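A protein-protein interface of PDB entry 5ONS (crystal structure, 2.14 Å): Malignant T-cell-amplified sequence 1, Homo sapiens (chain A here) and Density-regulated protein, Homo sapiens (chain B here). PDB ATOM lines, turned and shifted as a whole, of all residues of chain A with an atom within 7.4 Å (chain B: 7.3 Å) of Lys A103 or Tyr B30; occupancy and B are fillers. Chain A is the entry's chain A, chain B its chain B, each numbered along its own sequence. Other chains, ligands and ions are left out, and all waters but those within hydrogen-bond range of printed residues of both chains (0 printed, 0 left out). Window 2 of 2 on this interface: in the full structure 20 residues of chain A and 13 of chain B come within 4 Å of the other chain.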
ATOM      1  N   ASP A  98       6.947  23.822 -27.966  1.00  0.00           N
ATOM      2  CA  ASP A  98       6.145  24.759 -27.198  1.00  0.00           C
ATOM      3  C   ASP A  98       6.896  25.183 -25.939  1.00  0.00           C
ATOM      4  O   ASP A  98       7.734  24.446 -25.412  1.00  0.00           O
ATOM      5  CB  ASP A  98       4.796  24.136 -26.831  1.00  0.00           C
ATOM      6  CG  ASP A  98       4.901  23.099 -25.714  1.00  0.00           C
ATOM      7  OD1 ASP A  98       5.065  23.473 -24.533  1.00  0.00           O
ATOM      8  OD2 ASP A  98       4.797  21.896 -26.017  1.00  0.00           O
ATOM      9  N   LYS A  99       6.570  26.383 -25.446  1.00  0.00           N
ATOM     10  CA  LYS A  99       7.351  26.977 -24.364  1.00  0.00           C
ATOM     11  C   LYS A  99       7.335  26.114 -23.104  1.00  0.00           C
ATOM     12  O   LYS A  99       8.295  26.144 -22.329  1.00  0.00           O
ATOM     13  CB  LYS A  99       6.849  28.393 -24.055  1.00  0.00           C
ATOM     14  CG  LYS A  99       5.358  28.512 -23.736  1.00  0.00           C
ATOM     15  CD  LYS A  99       5.073  29.716 -22.830  1.00  0.00           C
ATOM     16  CE  LYS A  99       3.596  30.131 -22.855  1.00  0.00           C
ATOM     17  NZ  LYS A  99       3.026  30.384 -21.492  1.00  0.00           N
ATOM     18  N   GLY A 100       6.280  25.319 -22.896  1.00  0.00           N
ATOM     19  CA  GLY A 100       6.210  24.490 -21.701  1.00  0.00           C
ATOM     20  C   GLY A 100       7.299  23.438 -21.644  1.00  0.00           C
ATOM     21  O   GLY A 100       7.709  23.021 -20.558  1.00  0.00           O
ATOM     22  N   ALA A 101       7.801  23.014 -22.806  1.00  0.00           N
ATOM     23  CA  ALA A 101       8.818  21.976 -22.870  1.00  0.00           C
ATOM     24  C   ALA A 101      10.222  22.500 -22.591  1.00  0.00           C
ATOM     25  O   ALA A 101      11.131  21.686 -22.381  1.00  0.00           O
ATOM     26  CB  ALA A 101       8.781  21.294 -24.236  1.00  0.00           C
ATOM     27  N   ILE A 102      10.408  23.826 -22.549  1.00  0.00           N
ATOM     28  CA  ILE A 102      11.741  24.409 -22.374  1.00  0.00           C
ATOM     29  C   ILE A 102      12.397  23.886 -21.106  1.00  0.00           C
ATOM     30  O   ILE A 102      13.571  23.491 -21.110  1.00  0.00           O
ATOM     31  CB  ILE A 102      11.661  25.946 -22.356  1.00  0.00           C
ATOM     32  CG1 ILE A 102      11.247  26.479 -23.734  1.00  0.00           C
ATOM     33  CG2 ILE A 102      12.998  26.547 -21.908  1.00  0.00           C
ATOM     34  CD1 ILE A 102      11.094  27.992 -23.765  1.00  0.00           C
ATOM     35  N   LYS A 103      11.648  23.899 -19.994  1.00  0.00           N
ATOM     36  CA  LYS A 103      12.202  23.470 -18.716  1.00  0.00           C
ATOM     37  C   LYS A 103      12.671  22.034 -18.774  1.00  0.00           C
ATOM     38  O   LYS A 103      13.662  21.675 -18.129  1.00  0.00           O
ATOM     39  CB  LYS A 103      11.158  23.604 -17.610  1.00  0.00           C
ATOM     40  CG  LYS A 103      10.555  24.962 -17.525  1.00  0.00           C
ATOM     41  CD  LYS A 103       9.127  24.909 -17.971  1.00  0.00           C
ATOM     42  CE  LYS A 103       8.458  26.226 -17.678  1.00  0.00           C
ATOM     43  NZ  LYS A 103       7.341  26.483 -18.642  1.00  0.00           N
ATOM     44  N   PHE A 104      11.963  21.195 -19.526  1.00  0.00           N
ATOM     45  CA  PHE A 104      12.296  19.781 -19.520  1.00  0.00           C
ATOM     46  C   PHE A 104      13.502  19.484 -20.407  1.00  0.00           C
ATOM     47  O   PHE A 104      14.363  18.681 -20.023  1.00  0.00           O
ATOM     48  CB  PHE A 104      11.057  18.973 -19.902  1.00  0.00           C
ATOM     49  CG  PHE A 104       9.900  19.184 -18.941  1.00  0.00           C
ATOM     50  CD1 PHE A 104       9.059  20.281 -19.075  1.00  0.00           C
ATOM     51  CD2 PHE A 104       9.685  18.318 -17.885  1.00  0.00           C
ATOM     52  CE1 PHE A 104       8.014  20.493 -18.197  1.00  0.00           C
ATOM     53  CE2 PHE A 104       8.635  18.527 -17.002  1.00  0.00           C
ATOM     54  CZ  PHE A 104       7.801  19.618 -17.161  1.00  0.00           C
ATOM     55  N   VAL A 105      13.624  20.156 -21.558  1.00  0.00           N
ATOM     56  CA  VAL A 105      14.812  19.918 -22.381  1.00  0.00           C
ATOM     57  C   VAL A 105      16.057  20.566 -21.758  1.00  0.00           C
ATOM     58  O   VAL A 105      17.171  20.060 -21.941  1.00  0.00           O
ATOM     59  CB  VAL A 105      14.613  20.396 -23.834  1.00  0.00           C
ATOM     60  CG1 VAL A 105      13.297  19.892 -24.403  1.00  0.00           C
ATOM     61  CG2 VAL A 105      14.694  21.893 -23.931  1.00  0.00           C
ATOM     62  N   LEU A 106      15.911  21.673 -21.013  1.00  0.00           N
ATOM     63  CA  LEU A 106      17.066  22.232 -20.311  1.00  0.00           C
ATOM     64  C   LEU A 106      17.500  21.376 -19.132  1.00  0.00           C
ATOM     65  O   LEU A 106      18.582  21.615 -18.574  1.00  0.00           O
ATOM     66  CB  LEU A 106      16.778  23.655 -19.828  1.00  0.00           C
ATOM     67  CG  LEU A 106      16.786  24.733 -20.917  1.00  0.00           C
ATOM     68  CD1 LEU A 106      16.826  26.131 -20.305  1.00  0.00           C
ATOM     69  CD2 LEU A 106      17.948  24.523 -21.881  1.00  0.00           C
ATOM     70  N   SER A 107      16.682  20.408 -18.718  1.00  0.00           N
ATOM     71  CA  SER A 107      17.111  19.448 -17.715  1.00  0.00           C
ATOM     72  C   SER A 107      17.512  18.130 -18.353  1.00  0.00           C
ATOM     73  O   SER A 107      17.753  17.155 -17.642  1.00  0.00           O
ATOM     74  CB  SER A 107      16.029  19.237 -16.645  1.00  0.00           C
ATOM     75  OG  SER A 107      14.826  18.732 -17.205  1.00  0.00           O
ATOM     76  N   GLY A 108      17.622  18.095 -19.682  1.00  0.00           N
ATOM     77  CA  GLY A 108      18.189  16.962 -20.384  1.00  0.00           C
ATOM     78  C   GLY A 108      17.182  15.982 -20.936  1.00  0.00           C
ATOM     79  O   GLY A 108      17.588  14.964 -21.509  1.00  0.00           O
ATOM     80  N   ALA A 109      15.888  16.256 -20.789  1.00  0.00           N
ATOM     81  CA  ALA A 109      14.867  15.324 -21.238  1.00  0.00           C
ATOM     82  C   ALA A 109      14.798  15.281 -22.760  1.00  0.00           C
ATOM     83  O   ALA A 109      15.065  16.271 -23.451  1.00  0.00           O
ATOM     84  CB  ALA A 109      13.502  15.713 -20.672  1.00  0.00           C
ATOM     85  N   ALA A 136      12.684  27.437 -29.502  1.00  0.00           N
ATOM     86  CA  ALA A 136      11.648  27.508 -28.483  1.00  0.00           C
ATOM     87  C   ALA A 136      10.691  28.636 -28.821  1.00  0.00           C
ATOM     88  O   ALA A 136      11.129  29.759 -29.097  1.00  0.00           O
ATOM     89  CB  ALA A 136      12.245  27.720 -27.086  1.00  0.00           C
ATOM     90  N   GLU A 137       9.394  28.328 -28.803  1.00  0.00           N
ATOM     91  CA  GLU A 137       8.351  29.341 -28.888  1.00  0.00           C
ATOM     92  C   GLU A 137       8.716  30.565 -28.062  1.00  0.00           C
ATOM     93  O   GLU A 137       8.965  30.466 -26.855  1.00  0.00           O
ATOM     94  CB  GLU A 137       7.019  28.771 -28.402  1.00  0.00           C
ATOM     95  CG  GLU A 137       5.869  29.755 -28.566  1.00  0.00           C
ATOM     96  CD  GLU A 137       4.846  29.680 -27.447  1.00  0.00           C
ATOM     97  OE1 GLU A 137       4.639  28.577 -26.893  1.00  0.00           O
ATOM     98  OE2 GLU A 137       4.246  30.728 -27.125  1.00  0.00           O
ATOM     99  N   LYS A 139      11.445  32.302 -28.258  1.00  0.00           N
ATOM    100  CA  LYS A 139      12.874  32.469 -28.059  1.00  0.00           C
ATOM    101  C   LYS A 139      13.584  32.569 -29.400  1.00  0.00           C
ATOM    102  O   LYS A 139      13.236  31.870 -30.356  1.00  0.00           O
ATOM    103  CB  LYS A 139      13.438  31.325 -27.220  1.00  0.00           C
ATOM    104  CG  LYS A 139      12.875  31.305 -25.805  1.00  0.00           C
ATOM    105  CD  LYS A 139      13.311  32.531 -25.008  1.00  0.00           C
ATOM    106  CE  LYS A 139      12.392  32.798 -23.815  1.00  0.00           C
ATOM    107  NZ  LYS A 139      12.005  31.522 -23.167  1.00  0.00           N
ATOM    108  N   LEU A 143      18.206  26.095 -28.293  1.00  0.00           N
ATOM    109  CA  LEU A 143      18.488  25.601 -26.952  1.00  0.00           C
ATOM    110  C   LEU A 143      18.897  24.131 -26.923  1.00  0.00           C
ATOM    111  O   LEU A 143      19.211  23.610 -25.848  1.00  0.00           O
ATOM    112  CB  LEU A 143      17.269  25.822 -26.039  1.00  0.00           C
ATOM    113  CG  LEU A 143      16.141  24.782 -26.003  1.00  0.00           C
ATOM    114  CD1 LEU A 143      15.143  25.156 -24.939  1.00  0.00           C
ATOM    115  CD2 LEU A 143      15.439  24.682 -27.333  1.00  0.00           C
ATOM    116  N   CYS B  21      24.638  33.049 -15.437  1.00  0.00           N
ATOM    117  CA  CYS B  21      24.276  31.682 -15.795  1.00  0.00           C
ATOM    118  C   CYS B  21      24.897  31.207 -17.106  1.00  0.00           C
ATOM    119  O   CYS B  21      24.770  30.020 -17.426  1.00  0.00           O
ATOM    120  CB  CYS B  21      22.759  31.533 -15.861  1.00  0.00           C
ATOM    121  SG  CYS B  21      22.034  32.296 -17.335  1.00  0.00           S
ATOM    122  N   LEU B  23      24.028  31.663 -20.178  1.00  0.00           N
ATOM    123  CA  LEU B  23      23.015  31.417 -21.192  1.00  0.00           C
ATOM    124  C   LEU B  23      22.700  32.687 -21.965  1.00  0.00           C
ATOM    125  O   LEU B  23      23.026  33.789 -21.513  1.00  0.00           O
ATOM    126  CB  LEU B  23      21.755  30.880 -20.529  1.00  0.00           C
ATOM    127  CG  LEU B  23      21.728  29.369 -20.328  1.00  0.00           C
ATOM    128  CD1 LEU B  23      23.035  28.837 -19.777  1.00  0.00           C
ATOM    129  CD2 LEU B  23      20.617  29.038 -19.376  1.00  0.00           C
ATOM    130  N   GLU B  26      17.744  35.565 -22.824  1.00  0.00           N
ATOM    131  CA  GLU B  26      16.353  35.149 -22.927  1.00  0.00           C
ATOM    132  C   GLU B  26      16.079  33.826 -22.221  1.00  0.00           C
ATOM    133  O   GLU B  26      14.906  33.457 -22.076  1.00  0.00           O
ATOM    134  CB  GLU B  26      15.954  35.036 -24.401  1.00  0.00           C
ATOM    135  CG  GLU B  26      16.603  33.865 -25.106  1.00  0.00           C
ATOM    136  CD  GLU B  26      16.423  33.908 -26.615  1.00  0.00           C
ATOM    137  OE1 GLU B  26      17.190  33.218 -27.318  1.00  0.00           O
ATOM    138  OE2 GLU B  26      15.521  34.629 -27.100  1.00  0.00           O
ATOM    139  N   TYR B  27      17.124  33.099 -21.808  1.00  0.00           N
ATOM    140  CA  TYR B  27      16.991  31.873 -21.027  1.00  0.00           C
ATOM    141  C   TYR B  27      17.329  32.043 -19.550  1.00  0.00           C
ATOM    142  O   TYR B  27      17.184  31.078 -18.789  1.00  0.00           O
ATOM    143  CB  TYR B  27      17.875  30.767 -21.616  1.00  0.00           C
ATOM    144  CG  TYR B  27      17.340  30.304 -22.942  1.00  0.00           C
ATOM    145  CD1 TYR B  27      16.219  29.489 -22.994  1.00  0.00           C
ATOM    146  CD2 TYR B  27      17.922  30.714 -24.140  1.00  0.00           C
ATOM    147  CE1 TYR B  27      15.695  29.066 -24.191  1.00  0.00           C
ATOM    148  CE2 TYR B  27      17.401  30.286 -25.374  1.00  0.00           C
ATOM    149  CZ  TYR B  27      16.280  29.464 -25.382  1.00  0.00           C
ATOM    150  OH  TYR B  27      15.716  29.022 -26.558  1.00  0.00           O
ATOM    151  N   CYS B  28      17.788  33.228 -19.133  1.00  0.00           N
ATOM    152  CA  CYS B  28      18.013  33.514 -17.715  1.00  0.00           C
ATOM    153  C   CYS B  28      16.836  33.057 -16.865  1.00  0.00           C
ATOM    154  O   CYS B  28      17.016  32.464 -15.794  1.00  0.00           O
ATOM    155  CB  CYS B  28      18.232  35.014 -17.515  1.00  0.00           C
ATOM    156  SG  CYS B  28      19.811  35.653 -18.057  1.00  0.00           S
ATOM    157  N   GLU B  29      15.619  33.331 -17.343  1.00  0.00           N
ATOM    158  CA  GLU B  29      14.356  32.951 -16.718  1.00  0.00           C
ATOM    159  C   GLU B  29      14.371  31.542 -16.134  1.00  0.00           C
ATOM    160  O   GLU B  29      13.688  31.264 -15.143  1.00  0.00           O
ATOM    161  CB  GLU B  29      13.250  33.071 -17.759  1.00  0.00           C
ATOM    162  CG  GLU B  29      12.530  34.379 -17.711  1.00  0.00           C
ATOM    163  CD  GLU B  29      11.413  34.433 -18.716  1.00  0.00           C
ATOM    164  OE1 GLU B  29      10.318  34.931 -18.370  1.00  0.00           O
ATOM    165  OE2 GLU B  29      11.645  33.990 -19.866  1.00  0.00           O
ATOM    166  N   TYR B  30      15.158  30.652 -16.731  1.00  0.00           N
ATOM    167  CA  TYR B  30      15.143  29.232 -16.417  1.00  0.00           C
ATOM    168  C   TYR B  30      16.299  28.802 -15.522  1.00  0.00           C
ATOM    169  O   TYR B  30      16.392  27.616 -15.196  1.00  0.00           O
ATOM    170  CB  TYR B  30      15.145  28.419 -17.725  1.00  0.00           C
ATOM    171  CG  TYR B  30      13.945  28.745 -18.606  1.00  0.00           C
ATOM    172  CD1 TYR B  30      13.983  29.811 -19.508  1.00  0.00           C
ATOM    173  CD2 TYR B  30      12.767  28.008 -18.508  1.00  0.00           C
ATOM    174  CE1 TYR B  30      12.882  30.127 -20.297  1.00  0.00           C
ATOM    175  CE2 TYR B  30      11.659  28.317 -19.288  1.00  0.00           C
ATOM    176  CZ  TYR B  30      11.722  29.375 -20.182  1.00  0.00           C
ATOM    177  OH  TYR B  30      10.621  29.670 -20.953  1.00  0.00           O
ATOM    178  N   MET B  31      17.161  29.727 -15.101  1.00  0.00           N
ATOM    179  CA  MET B  31      18.325  29.393 -14.271  1.00  0.00           C
ATOM    180  C   MET B  31      18.295  30.163 -12.956  1.00  0.00           C
ATOM    181  O   MET B  31      18.467  31.397 -12.959  1.00  0.00           O
ATOM    182  CB  MET B  31      19.614  29.690 -15.034  1.00  0.00           C
ATOM    183  CG  MET B  31      19.681  28.984 -16.392  1.00  0.00           C
ATOM    184  SD  MET B  31      20.424  27.332 -16.361  1.00  0.00           S
ATOM    185  CE  MET B  31      19.155  26.295 -17.101  1.00  0.00           C
ATOM    186  N   PRO B  32      18.087  29.498 -11.811  1.00  0.00           N
ATOM    187  CA  PRO B  32      18.055  30.145 -10.487  1.00  0.00           C
ATOM    188  C   PRO B  32      19.407  30.721 -10.062  1.00  0.00           C
ATOM    189  O   PRO B  32      19.468  31.476  -9.092  1.00  0.00           O
ATOM    190  CB  PRO B  32      17.637  29.008  -9.549  1.00  0.00           C
ATOM    191  CG  PRO B  32      18.023  27.754 -10.271  1.00  0.00           C
ATOM    192  CD  PRO B  32      17.825  28.051 -11.732  1.00  0.00           C
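The side-chain amino group (NZ) of Lys A139 lies within hydrogen-bond range of the side-chain hydroxyl (OH) of Tyr B30 (3.2 Å).
The side-chain hydroxyl (OG) of Ser A107 is in hydrogen-bond range of the backbone carbonyl oxygen (O) of Lys A103 (3.3 Å).
Among the printed residues, merely in contact across the chains: Lys A139 with Glu B26, Lys A139 with Tyr B27, Ile A102 with Tyr B30, Leu A143 with Tyr B27, Ala A136 with Tyr B27, Leu A106 with Tyr B30, Lys A103 with Tyr B30 and Leu A106 with Met B31.
Lys A103 touches just one residue of chain B: Tyr B30 (3.9 Å).
Tyr B30 touches four residues of chain A.
Printed residues of chain A within 4 Å of Tyr B27: Ala A136, Lys A139 and Leu A143.
Printed residues of chain A within 4 Å of Met B31: Leu A106 (3.96 Å).
Of the printed residues of chain B, Ile A102 touches Tyr B30.
Of the printed residues of chain B, Leu A106 touches Tyr B30 (3.8 Å) and Met B31 (3.96 Å).
Of the printed residues of chain B, Ala A136 touches Tyr B27 (3.7 Å).
Cys B28 touches none of the printed residues of chain A.
Asp A98 touches none of the printed residues of chain B.
The nearest printed residue of chain B that does not touch Lys A103 is Met B31 (7.3 Å).
The nearest printed residue of chain B that does not touch Lys A139 is Glu B29 (4.1 Å).
Hydrophobic or aromatic side chains of chain B within 4 Å of the printed part of chain A: Tyr B27, Tyr B30 and Met B31.
Of the 16 printed residues of chain A, 6 touch a printed residue of chain B.
Among the printed residues, 9 pairs touch across the chains.
Among the printed residues, no Asp or Glu carboxylate lies within 4 Å of a Lys or Arg side-chain nitrogen of the other chain.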
